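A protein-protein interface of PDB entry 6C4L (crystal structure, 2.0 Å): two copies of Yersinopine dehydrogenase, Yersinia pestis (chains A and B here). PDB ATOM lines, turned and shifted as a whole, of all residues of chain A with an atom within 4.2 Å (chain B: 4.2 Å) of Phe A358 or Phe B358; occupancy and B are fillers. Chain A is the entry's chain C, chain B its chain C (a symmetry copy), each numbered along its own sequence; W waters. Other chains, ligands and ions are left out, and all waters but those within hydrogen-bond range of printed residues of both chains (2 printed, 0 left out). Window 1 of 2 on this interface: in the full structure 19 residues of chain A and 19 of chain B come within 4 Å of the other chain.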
ATOM      1  N   VAL A 292       3.551 -17.828 -17.083  1.00  0.00           N
ATOM      2  CA  VAL A 292       3.537 -16.372 -16.915  1.00  0.00           C
ATOM      3  C   VAL A 292       3.186 -15.701 -18.232  1.00  0.00           C
ATOM      4  O   VAL A 292       3.802 -15.961 -19.271  1.00  0.00           O
ATOM      5  CB  VAL A 292       4.873 -15.862 -16.351  1.00  0.00           C
ATOM      6  CG1 VAL A 292       4.846 -14.331 -16.206  1.00  0.00           C
ATOM      7  CG2 VAL A 292       5.136 -16.508 -15.014  1.00  0.00           C
ATOM      8  N   CYS A 293       2.188 -14.829 -18.181  1.00  0.00           N
ATOM      9  CA  CYS A 293       1.681 -14.065 -19.300  1.00  0.00           C
ATOM     10  C   CYS A 293       0.729 -13.035 -18.718  1.00  0.00           C
ATOM     11  O   CYS A 293       0.406 -13.097 -17.535  1.00  0.00           O
ATOM     12  CB  CYS A 293       0.956 -14.968 -20.311  1.00  0.00           C
ATOM     13  SG  CYS A 293      -0.510 -15.819 -19.626  1.00  0.00           S
ATOM     14  N   ILE A 297      -0.849 -13.011 -14.824  1.00  0.00           N
ATOM     15  CA  ILE A 297      -0.523 -11.876 -13.973  1.00  0.00           C
ATOM     16  C   ILE A 297      -1.779 -11.146 -13.537  1.00  0.00           C
ATOM     17  O   ILE A 297      -1.841 -10.594 -12.428  1.00  0.00           O
ATOM     18  CB  ILE A 297       0.436 -10.921 -14.714  1.00  0.00           C
ATOM     19  CG1 ILE A 297       1.839 -11.548 -14.824  1.00  0.00           C
ATOM     20  CG2 ILE A 297       0.426  -9.561 -14.037  1.00  0.00           C
ATOM     21  CD1 ILE A 297       2.520 -11.877 -13.517  1.00  0.00           C
ATOM     22  N   MET A 336      14.371  -2.555 -13.180  1.00  0.00           N
ATOM     23  CA  MET A 336      13.222  -3.309 -13.669  1.00  0.00           C
ATOM     24  C   MET A 336      11.966  -2.915 -12.906  1.00  0.00           C
ATOM     25  O   MET A 336      11.024  -2.396 -13.507  1.00  0.00           O
ATOM     26  CB  MET A 336      13.476  -4.814 -13.567  1.00  0.00           C
ATOM     27  CG  MET A 336      14.644  -5.280 -14.418  1.00  0.00           C
ATOM     28  SD  MET A 336      14.236  -5.229 -16.199  1.00  0.00           S
ATOM     29  CE  MET A 336      13.233  -6.697 -16.359  1.00  0.00           C
ATOM     30  N   GLN A 354      -0.401  -4.750 -12.812  1.00  0.00           N
ATOM     31  CA  GLN A 354      -0.093  -5.944 -13.583  1.00  0.00           C
ATOM     32  C   GLN A 354       1.215  -5.778 -14.333  1.00  0.00           C
ATOM     33  O   GLN A 354       2.092  -6.656 -14.293  1.00  0.00           O
ATOM     34  CB  GLN A 354      -1.240  -6.237 -14.542  1.00  0.00           C
ATOM     35  CG  GLN A 354      -2.509  -6.696 -13.821  1.00  0.00           C
ATOM     36  CD  GLN A 354      -3.711  -6.747 -14.762  1.00  0.00           C
ATOM     37  OE1 GLN A 354      -3.572  -7.031 -15.957  1.00  0.00           O
ATOM     38  NE2 GLN A 354      -4.881  -6.440 -14.238  1.00  0.00           N
ATOM     39  N   TYR A 355       1.375  -4.643 -15.009  1.00  0.00           N
ATOM     40  CA  TYR A 355       2.661  -4.353 -15.625  1.00  0.00           C
ATOM     41  C   TYR A 355       3.788  -4.579 -14.618  1.00  0.00           C
ATOM     42  O   TYR A 355       4.727  -5.345 -14.873  1.00  0.00           O
ATOM     43  CB  TYR A 355       2.636  -2.926 -16.191  1.00  0.00           C
ATOM     44  CG  TYR A 355       3.836  -2.528 -17.022  1.00  0.00           C
ATOM     45  CD1 TYR A 355       4.735  -3.479 -17.513  1.00  0.00           C
ATOM     46  CD2 TYR A 355       4.058  -1.194 -17.334  1.00  0.00           C
ATOM     47  CE1 TYR A 355       5.830  -3.094 -18.297  1.00  0.00           C
ATOM     48  CE2 TYR A 355       5.151  -0.808 -18.111  1.00  0.00           C
ATOM     49  CZ  TYR A 355       6.032  -1.761 -18.570  1.00  0.00           C
ATOM     50  OH  TYR A 355       7.105  -1.383 -19.318  1.00  0.00           O
ATOM     51  N   ALA A 356       3.665  -4.002 -13.417  1.00  0.00           N
ATOM     52  CA  ALA A 356       4.763  -4.113 -12.460  1.00  0.00           C
ATOM     53  C   ALA A 356       5.022  -5.568 -12.097  1.00  0.00           C
ATOM     54  O   ALA A 356       6.181  -6.001 -11.978  1.00  0.00           O
ATOM     55  CB  ALA A 356       4.479  -3.285 -11.196  1.00  0.00           C
ATOM     56  N   LEU A 357       3.948  -6.336 -11.893  1.00  0.00           N
ATOM     57  CA  LEU A 357       4.099  -7.734 -11.547  1.00  0.00           C
ATOM     58  C   LEU A 357       4.709  -8.532 -12.680  1.00  0.00           C
ATOM     59  O   LEU A 357       5.562  -9.394 -12.439  1.00  0.00           O
ATOM     60  CB  LEU A 357       2.739  -8.310 -11.162  1.00  0.00           C
ATOM     61  CG  LEU A 357       2.281  -7.954  -9.746  1.00  0.00           C
ATOM     62  CD1 LEU A 357       0.823  -8.342  -9.584  1.00  0.00           C
ATOM     63  CD2 LEU A 357       3.169  -8.661  -8.765  1.00  0.00           C
ATOM     64  N   PHE A 358       4.266  -8.284 -13.934  1.00  0.00           N
ATOM     65  CA  PHE A 358       4.868  -8.996 -15.048  1.00  0.00           C
ATOM     66  C   PHE A 358       6.355  -8.725 -15.109  1.00  0.00           C
ATOM     67  O   PHE A 358       7.156  -9.647 -15.294  1.00  0.00           O
ATOM     68  CB  PHE A 358       4.215  -8.607 -16.378  1.00  0.00           C
ATOM     69  CG  PHE A 358       4.737  -9.400 -17.534  1.00  0.00           C
ATOM     70  CD1 PHE A 358       5.818  -8.959 -18.255  1.00  0.00           C
ATOM     71  CD2 PHE A 358       4.153 -10.620 -17.882  1.00  0.00           C
ATOM     72  CE1 PHE A 358       6.306  -9.706 -19.333  1.00  0.00           C
ATOM     73  CE2 PHE A 358       4.629 -11.352 -18.936  1.00  0.00           C
ATOM     74  CZ  PHE A 358       5.718 -10.874 -19.675  1.00  0.00           C
ATOM     75  N   VAL A 359       6.744  -7.460 -14.955  1.00  0.00           N
ATOM     76  CA  VAL A 359       8.167  -7.107 -14.977  1.00  0.00           C
ATOM     77  C   VAL A 359       8.893  -7.838 -13.853  1.00  0.00           C
ATOM     78  O   VAL A 359       9.943  -8.465 -14.064  1.00  0.00           O
ATOM     79  CB  VAL A 359       8.346  -5.574 -14.883  1.00  0.00           C
ATOM     80  CG1 VAL A 359       9.824  -5.182 -14.727  1.00  0.00           C
ATOM     81  CG2 VAL A 359       7.802  -4.826 -16.130  1.00  0.00           C
ATOM     82  N   ARG A 360       8.317  -7.807 -12.648  1.00  0.00           N
ATOM     83  CA  ARG A 360       8.925  -8.524 -11.528  1.00  0.00           C
ATOM     84  C   ARG A 360       9.216  -9.977 -11.891  1.00  0.00           C
ATOM     85  O   ARG A 360      10.340 -10.457 -11.711  1.00  0.00           O
ATOM     86  CB  ARG A 360       8.007  -8.453 -10.312  1.00  0.00           C
ATOM     87  CG  ARG A 360       8.692  -8.760  -9.000  1.00  0.00           C
ATOM     88  CD  ARG A 360       8.056  -9.902  -8.313  1.00  0.00           C
ATOM     89  NE  ARG A 360       8.906 -10.351  -7.228  1.00  0.00           N
ATOM     90  CZ  ARG A 360       8.792 -11.513  -6.605  1.00  0.00           C
ATOM     91  NH1 ARG A 360       7.844 -12.386  -6.958  1.00  0.00           N
ATOM     92  NH2 ARG A 360       9.640 -11.802  -5.624  1.00  0.00           N
ATOM     93  N   TYR A 361       8.220 -10.700 -12.427  1.00  0.00           N
ATOM     94  CA  TYR A 361       8.439 -12.121 -12.686  1.00  0.00           C
ATOM     95  C   TYR A 361       9.358 -12.351 -13.868  1.00  0.00           C
ATOM     96  O   TYR A 361      10.063 -13.368 -13.914  1.00  0.00           O
ATOM     97  CB  TYR A 361       7.102 -12.849 -12.867  1.00  0.00           C
ATOM     98  CG  TYR A 361       6.547 -13.162 -11.504  1.00  0.00           C
ATOM     99  CD1 TYR A 361       7.069 -14.210 -10.759  1.00  0.00           C
ATOM    100  CD2 TYR A 361       5.586 -12.357 -10.916  1.00  0.00           C
ATOM    101  CE1 TYR A 361       6.618 -14.480  -9.484  1.00  0.00           C
ATOM    102  CE2 TYR A 361       5.133 -12.615  -9.622  1.00  0.00           C
ATOM    103  CZ  TYR A 361       5.654 -13.681  -8.916  1.00  0.00           C
ATOM    104  OH  TYR A 361       5.213 -13.967  -7.631  1.00  0.00           O
ATOM    105  N   THR A 362       9.378 -11.433 -14.827  1.00  0.00           N
ATOM    106  CA  THR A 362      10.393 -11.519 -15.870  1.00  0.00           C
ATOM    107  C   THR A 362      11.783 -11.340 -15.289  1.00  0.00           C
ATOM    108  O   THR A 362      12.698 -12.104 -15.616  1.00  0.00           O
ATOM    109  CB  THR A 362      10.128 -10.479 -16.956  1.00  0.00           C
ATOM    110  OG1 THR A 362       8.831 -10.708 -17.497  1.00  0.00           O
ATOM    111  CG2 THR A 362      11.172 -10.556 -18.111  1.00  0.00           C
ATOM    112  N   VAL B 292      16.624  -3.967 -22.023  1.00  0.00           N
ATOM    113  CA  VAL B 292      15.161  -3.940 -21.942  1.00  0.00           C
ATOM    114  C   VAL B 292      14.724  -3.821 -20.491  1.00  0.00           C
ATOM    115  O   VAL B 292      15.142  -4.598 -19.627  1.00  0.00           O
ATOM    116  CB  VAL B 292      14.542  -5.170 -22.626  1.00  0.00           C
ATOM    117  CG1 VAL B 292      13.009  -5.135 -22.508  1.00  0.00           C
ATOM    118  CG2 VAL B 292      14.953  -5.199 -24.077  1.00  0.00           C
ATOM    119  N   CYS B 293      13.873  -2.837 -20.231  1.00  0.00           N
ATOM    120  CA  CYS B 293      13.314  -2.532 -18.932  1.00  0.00           C
ATOM    121  C   CYS B 293      12.218  -1.507 -19.169  1.00  0.00           C
ATOM    122  O   CYS B 293      12.089  -0.992 -20.275  1.00  0.00           O
ATOM    123  CB  CYS B 293      14.384  -1.976 -17.979  1.00  0.00           C
ATOM    124  SG  CYS B 293      15.134  -0.407 -18.544  1.00  0.00           S
ATOM    125  N   ILE B 297      11.576   0.696 -22.689  1.00  0.00           N
ATOM    126  CA  ILE B 297      10.311   0.503 -23.381  1.00  0.00           C
ATOM    127  C   ILE B 297       9.540   1.807 -23.475  1.00  0.00           C
ATOM    128  O   ILE B 297       8.813   2.047 -24.451  1.00  0.00           O
ATOM    129  CB  ILE B 297       9.475  -0.576 -22.661  1.00  0.00           C
ATOM    130  CG1 ILE B 297      10.087  -1.971 -22.891  1.00  0.00           C
ATOM    131  CG2 ILE B 297       8.022  -0.468 -23.090  1.00  0.00           C
ATOM    132  CD1 ILE B 297      10.183  -2.421 -24.328  1.00  0.00           C
ATOM    133  N   MET B 336       0.732 -14.151 -25.070  1.00  0.00           N
ATOM    134  CA  MET B 336       1.577 -13.091 -24.530  1.00  0.00           C
ATOM    135  C   MET B 336       1.083 -11.730 -24.998  1.00  0.00           C
ATOM    136  O   MET B 336       0.687 -10.906 -24.171  1.00  0.00           O
ATOM    137  CB  MET B 336       3.039 -13.308 -24.921  1.00  0.00           C
ATOM    138  CG  MET B 336       3.620 -14.596 -24.365  1.00  0.00           C
ATOM    139  SD  MET B 336       3.871 -14.491 -22.558  1.00  0.00           S
ATOM    140  CE  MET B 336       5.363 -13.512 -22.480  1.00  0.00           C
ATOM    141  N   GLN B 354       3.089   0.500 -23.344  1.00  0.00           N
ATOM    142  CA  GLN B 354       4.389   0.080 -22.844  1.00  0.00           C
ATOM    143  C   GLN B 354       4.328  -1.336 -22.305  1.00  0.00           C
ATOM    144  O   GLN B 354       5.171  -2.184 -22.635  1.00  0.00           O
ATOM    145  CB  GLN B 354       4.856   1.055 -21.771  1.00  0.00           C
ATOM    146  CG  GLN B 354       5.212   2.432 -22.337  1.00  0.00           C
ATOM    147  CD  GLN B 354       5.439   3.460 -21.232  1.00  0.00           C
ATOM    148  OE1 GLN B 354       5.914   3.128 -20.141  1.00  0.00           O
ATOM    149  NE2 GLN B 354       5.069   4.698 -21.497  1.00  0.00           N
ATOM    150  N   TYR B 355       3.318  -1.618 -21.485  1.00  0.00           N
ATOM    151  CA  TYR B 355       3.112  -2.992 -21.051  1.00  0.00           C
ATOM    152  C   TYR B 355       3.148  -3.933 -22.255  1.00  0.00           C
ATOM    153  O   TYR B 355       3.930  -4.893 -22.290  1.00  0.00           O
ATOM    154  CB  TYR B 355       1.799  -3.077 -20.260  1.00  0.00           C
ATOM    155  CG  TYR B 355       1.523  -4.402 -19.585  1.00  0.00           C
ATOM    156  CD1 TYR B 355       2.526  -5.361 -19.415  1.00  0.00           C
ATOM    157  CD2 TYR B 355       0.255  -4.688 -19.096  1.00  0.00           C
ATOM    158  CE1 TYR B 355       2.258  -6.575 -18.770  1.00  0.00           C
ATOM    159  CE2 TYR B 355      -0.015  -5.899 -18.459  1.00  0.00           C
ATOM    160  CZ  TYR B 355       0.986  -6.833 -18.316  1.00  0.00           C
ATOM    161  OH  TYR B 355       0.719  -8.020 -17.704  1.00  0.00           O
ATOM    162  N   ALA B 356       2.383  -3.618 -23.306  1.00  0.00           N
ATOM    163  CA  ALA B 356       2.315  -4.541 -24.437  1.00  0.00           C
ATOM    164  C   ALA B 356       3.684  -4.720 -25.074  1.00  0.00           C
ATOM    165  O   ALA B 356       4.071  -5.838 -25.454  1.00  0.00           O
ATOM    166  CB  ALA B 356       1.294  -4.059 -25.480  1.00  0.00           C
ATOM    167  N   LEU B 357       4.425  -3.619 -25.222  1.00  0.00           N
ATOM    168  CA  LEU B 357       5.745  -3.695 -25.816  1.00  0.00           C
ATOM    169  C   LEU B 357       6.708  -4.476 -24.948  1.00  0.00           C
ATOM    170  O   LEU B 357       7.504  -5.268 -25.468  1.00  0.00           O
ATOM    171  CB  LEU B 357       6.272  -2.284 -26.060  1.00  0.00           C
ATOM    172  CG  LEU B 357       5.695  -1.600 -27.302  1.00  0.00           C
ATOM    173  CD1 LEU B 357       6.075  -0.131 -27.282  1.00  0.00           C
ATOM    174  CD2 LEU B 357       6.213  -2.306 -28.520  1.00  0.00           C
ATOM    175  N   PHE B 358       6.680  -4.251 -23.615  1.00  0.00           N
ATOM    176  CA  PHE B 358       7.556  -5.022 -22.750  1.00  0.00           C
ATOM    177  C   PHE B 358       7.274  -6.501 -22.892  1.00  0.00           C
ATOM    178  O   PHE B 358       8.199  -7.312 -22.999  1.00  0.00           O
ATOM    179  CB  PHE B 358       7.404  -4.603 -21.285  1.00  0.00           C
ATOM    180  CG  PHE B 358       8.368  -5.302 -20.379  1.00  0.00           C
ATOM    181  CD1 PHE B 358       8.035  -6.492 -19.784  1.00  0.00           C
ATOM    182  CD2 PHE B 358       9.639  -4.771 -20.147  1.00  0.00           C
ATOM    183  CE1 PHE B 358       8.941  -7.145 -18.942  1.00  0.00           C
ATOM    184  CE2 PHE B 358      10.527  -5.407 -19.323  1.00  0.00           C
ATOM    185  CZ  PHE B 358      10.161  -6.609 -18.706  1.00  0.00           C
ATOM    186  N   VAL B 359       5.994  -6.873 -22.897  1.00  0.00           N
ATOM    187  CA  VAL B 359       5.625  -8.284 -23.052  1.00  0.00           C
ATOM    188  C   VAL B 359       6.147  -8.804 -24.386  1.00  0.00           C
ATOM    189  O   VAL B 359       6.782  -9.868 -24.460  1.00  0.00           O
ATOM    190  CB  VAL B 359       4.095  -8.460 -22.918  1.00  0.00           C
ATOM    191  CG1 VAL B 359       3.657  -9.896 -23.250  1.00  0.00           C
ATOM    192  CG2 VAL B 359       3.573  -8.140 -21.492  1.00  0.00           C
ATOM    193  N   ARG B 360       5.926  -8.037 -25.458  1.00  0.00           N
ATOM    194  CA  ARG B 360       6.437  -8.442 -26.766  1.00  0.00           C
ATOM    195  C   ARG B 360       7.925  -8.774 -26.703  1.00  0.00           C
ATOM    196  O   ARG B 360       8.350  -9.846 -27.144  1.00  0.00           O
ATOM    197  CB  ARG B 360       6.182  -7.335 -27.784  1.00  0.00           C
ATOM    198  CG  ARG B 360       6.255  -7.789 -29.224  1.00  0.00           C
ATOM    199  CD  ARG B 360       7.278  -7.036 -29.976  1.00  0.00           C
ATOM    200  NE  ARG B 360       7.526  -7.688 -31.247  1.00  0.00           N
ATOM    201  CZ  ARG B 360       8.571  -7.460 -32.026  1.00  0.00           C
ATOM    202  NH1 ARG B 360       9.506  -6.575 -31.672  1.00  0.00           N
ATOM    203  NH2 ARG B 360       8.679  -8.130 -33.169  1.00  0.00           N
ATOM    204  N   TYR B 361       8.744  -7.872 -26.137  1.00  0.00           N
ATOM    205  CA  TYR B 361      10.184  -8.117 -26.158  1.00  0.00           C
ATOM    206  C   TYR B 361      10.591  -9.217 -25.200  1.00  0.00           C
ATOM    207  O   TYR B 361      11.589  -9.908 -25.441  1.00  0.00           O
ATOM    208  CB  TYR B 361      10.955  -6.821 -25.881  1.00  0.00           C
ATOM    209  CG  TYR B 361      11.047  -6.044 -27.166  1.00  0.00           C
ATOM    210  CD1 TYR B 361      11.948  -6.423 -28.151  1.00  0.00           C
ATOM    211  CD2 TYR B 361      10.172  -5.006 -27.445  1.00  0.00           C
ATOM    212  CE1 TYR B 361      12.011  -5.763 -29.361  1.00  0.00           C
ATOM    213  CE2 TYR B 361      10.221  -4.342 -28.670  1.00  0.00           C
ATOM    214  CZ  TYR B 361      11.145  -4.727 -29.621  1.00  0.00           C
ATOM    215  OH  TYR B 361      11.222  -4.075 -30.844  1.00  0.00           O
ATOM    216  N   THR B 362       9.845  -9.406 -24.119  1.00  0.00           N
ATOM    217  CA  THR B 362      10.085 -10.580 -23.287  1.00  0.00           C
ATOM    218  C   THR B 362       9.789 -11.855 -24.052  1.00  0.00           C
ATOM    219  O   THR B 362      10.580 -12.804 -24.013  1.00  0.00           O
ATOM    220  CB  THR B 362       9.244 -10.510 -22.014  1.00  0.00           C
ATOM    221  OG1 THR B 362       9.582  -9.319 -21.311  1.00  0.00           O
ATOM    222  CG2 THR B 362       9.494 -11.731 -21.077  1.00  0.00           C
HETATM  223  O   HOH W   1       7.521   1.276 -19.657  1.00  0.00           O
HETATM  224  O   HOH W   2      -1.854  -8.515 -17.002  1.00  0.00           O
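The backbone carbonyl oxygen (O) of Val A292 lies close to the side-chain sulfur (SD) of Met B336 (3.6 Å). SD of Met A336 sits close to O of Val B292 (3.6 Å).
O of Phe A358 lies within hydrogen-bond range of OG1 of Thr A362, 3.0 Å away. The backbone carbonyl oxygen (O) of Phe B358 sits at hydrogen-bond distance from the side-chain hydroxyl (OG1) of Thr B362 (3.0 Å).
Among the printed residues, merely in contact across the chains: Cys A293 with Met B336 (3.7 Å), Ile A297 with Tyr B355 (3.99 Å), Met A336 with Cys B293 (3.7 Å), Met A336 with Phe B358 (3.9 Å), Gln A354 with Tyr B355 (3.9 Å), Tyr A355 with Ile B297 (3.99 Å), Tyr A355 with Gln B354 (3.9 Å), Tyr A355 with Tyr B355 (3.5 Å), Tyr A355 with Phe B358 (3.7 Å), Phe A358 with Met B336 (3.9 Å), Phe A358 with Tyr B355 (3.7 Å), Phe A358 with Phe B358 (3.7 Å), Phe A358 with Val B359 (3.8 Å), Phe A358 with Thr B362 (3.8 Å), Val A359 with Phe B358 (3.8 Å), Thr A362 with Phe B358 (3.8 Å) and Thr A362 with Thr B362 (3.6 Å).
Printed residues of chain B within 4 Å of Cys A293: Met B336. Printed residues of chain B within 4 Å of Met A336: Val B292 (3.6 Å), Cys B293 (3.7 Å) and Phe B358 (3.9 Å). Printed residues of chain B within 4 Å of Phe A358: Met B336 (3.9 Å), Tyr B355 (3.7 Å), Phe B358 (3.7 Å), Val B359 (3.8 Å) and Thr B362 (3.8 Å). Arg A360 touches none of the printed residues of chain B. Of the printed residues of chain B, Thr A362 touches Phe B358 (3.8 Å) and Thr B362 (3.6 Å). Of the printed residues of chain A, Ile B297 touches Tyr A355. Of the printed residues of chain A, Tyr B355 touches Ile A297 (3.99 Å), Gln A354 (3.9 Å), Tyr A355 (3.5 Å) and Phe A358 (3.7 Å). Leu B357 touches none of the printed residues of chain A. Phe B358 touches just these residues of chain A: Met A336, Tyr A355, Phe A358, Val A359 and Thr A362. The nearest printed residue of chain B that does not touch Phe A358 is Arg B360 (6.4 Å). The nearest printed residue of chain B that does not touch Val A359 is Tyr B355 (6.0 Å).
Of the 13 printed residues of chain B, 9 touch a printed residue of chain A. Along chain B the printed residues that touch a printed residue of chain A span positions 292 to 362. Of the 13 printed residues of chain A, 9 touch a printed residue of chain B. Hydrophobic or aromatic side chains of chain A that line the printed part of chain B: Ile A297, Met A336, Tyr A355, Phe A358 and Val A359.
Gln A354 touches Tyr B355, and with the chains exchanged Tyr A355 touches Gln B354. Tyr A355 touches Phe B358, and with the chains exchanged Phe A358 touches Tyr B355. Phe A358 touches its own counterpart, Phe B358. Phe A358 touches Val B359, and with the chains exchanged Val A359 touches Phe B358. Positions printed for both chains: 292, 293, 297, 336, 354, 355, 356, 357, 358, 359, 360, 361 and 362. Of the 19 pairs that touch across the chains among the printed residues, 19 have their exchanged pair printed and touching as well.
Water W2 bridges OE1 of Gln A354 and OH of Tyr B355. Water W1 bridges OE1 of Gln B354 and OH of Tyr A355.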
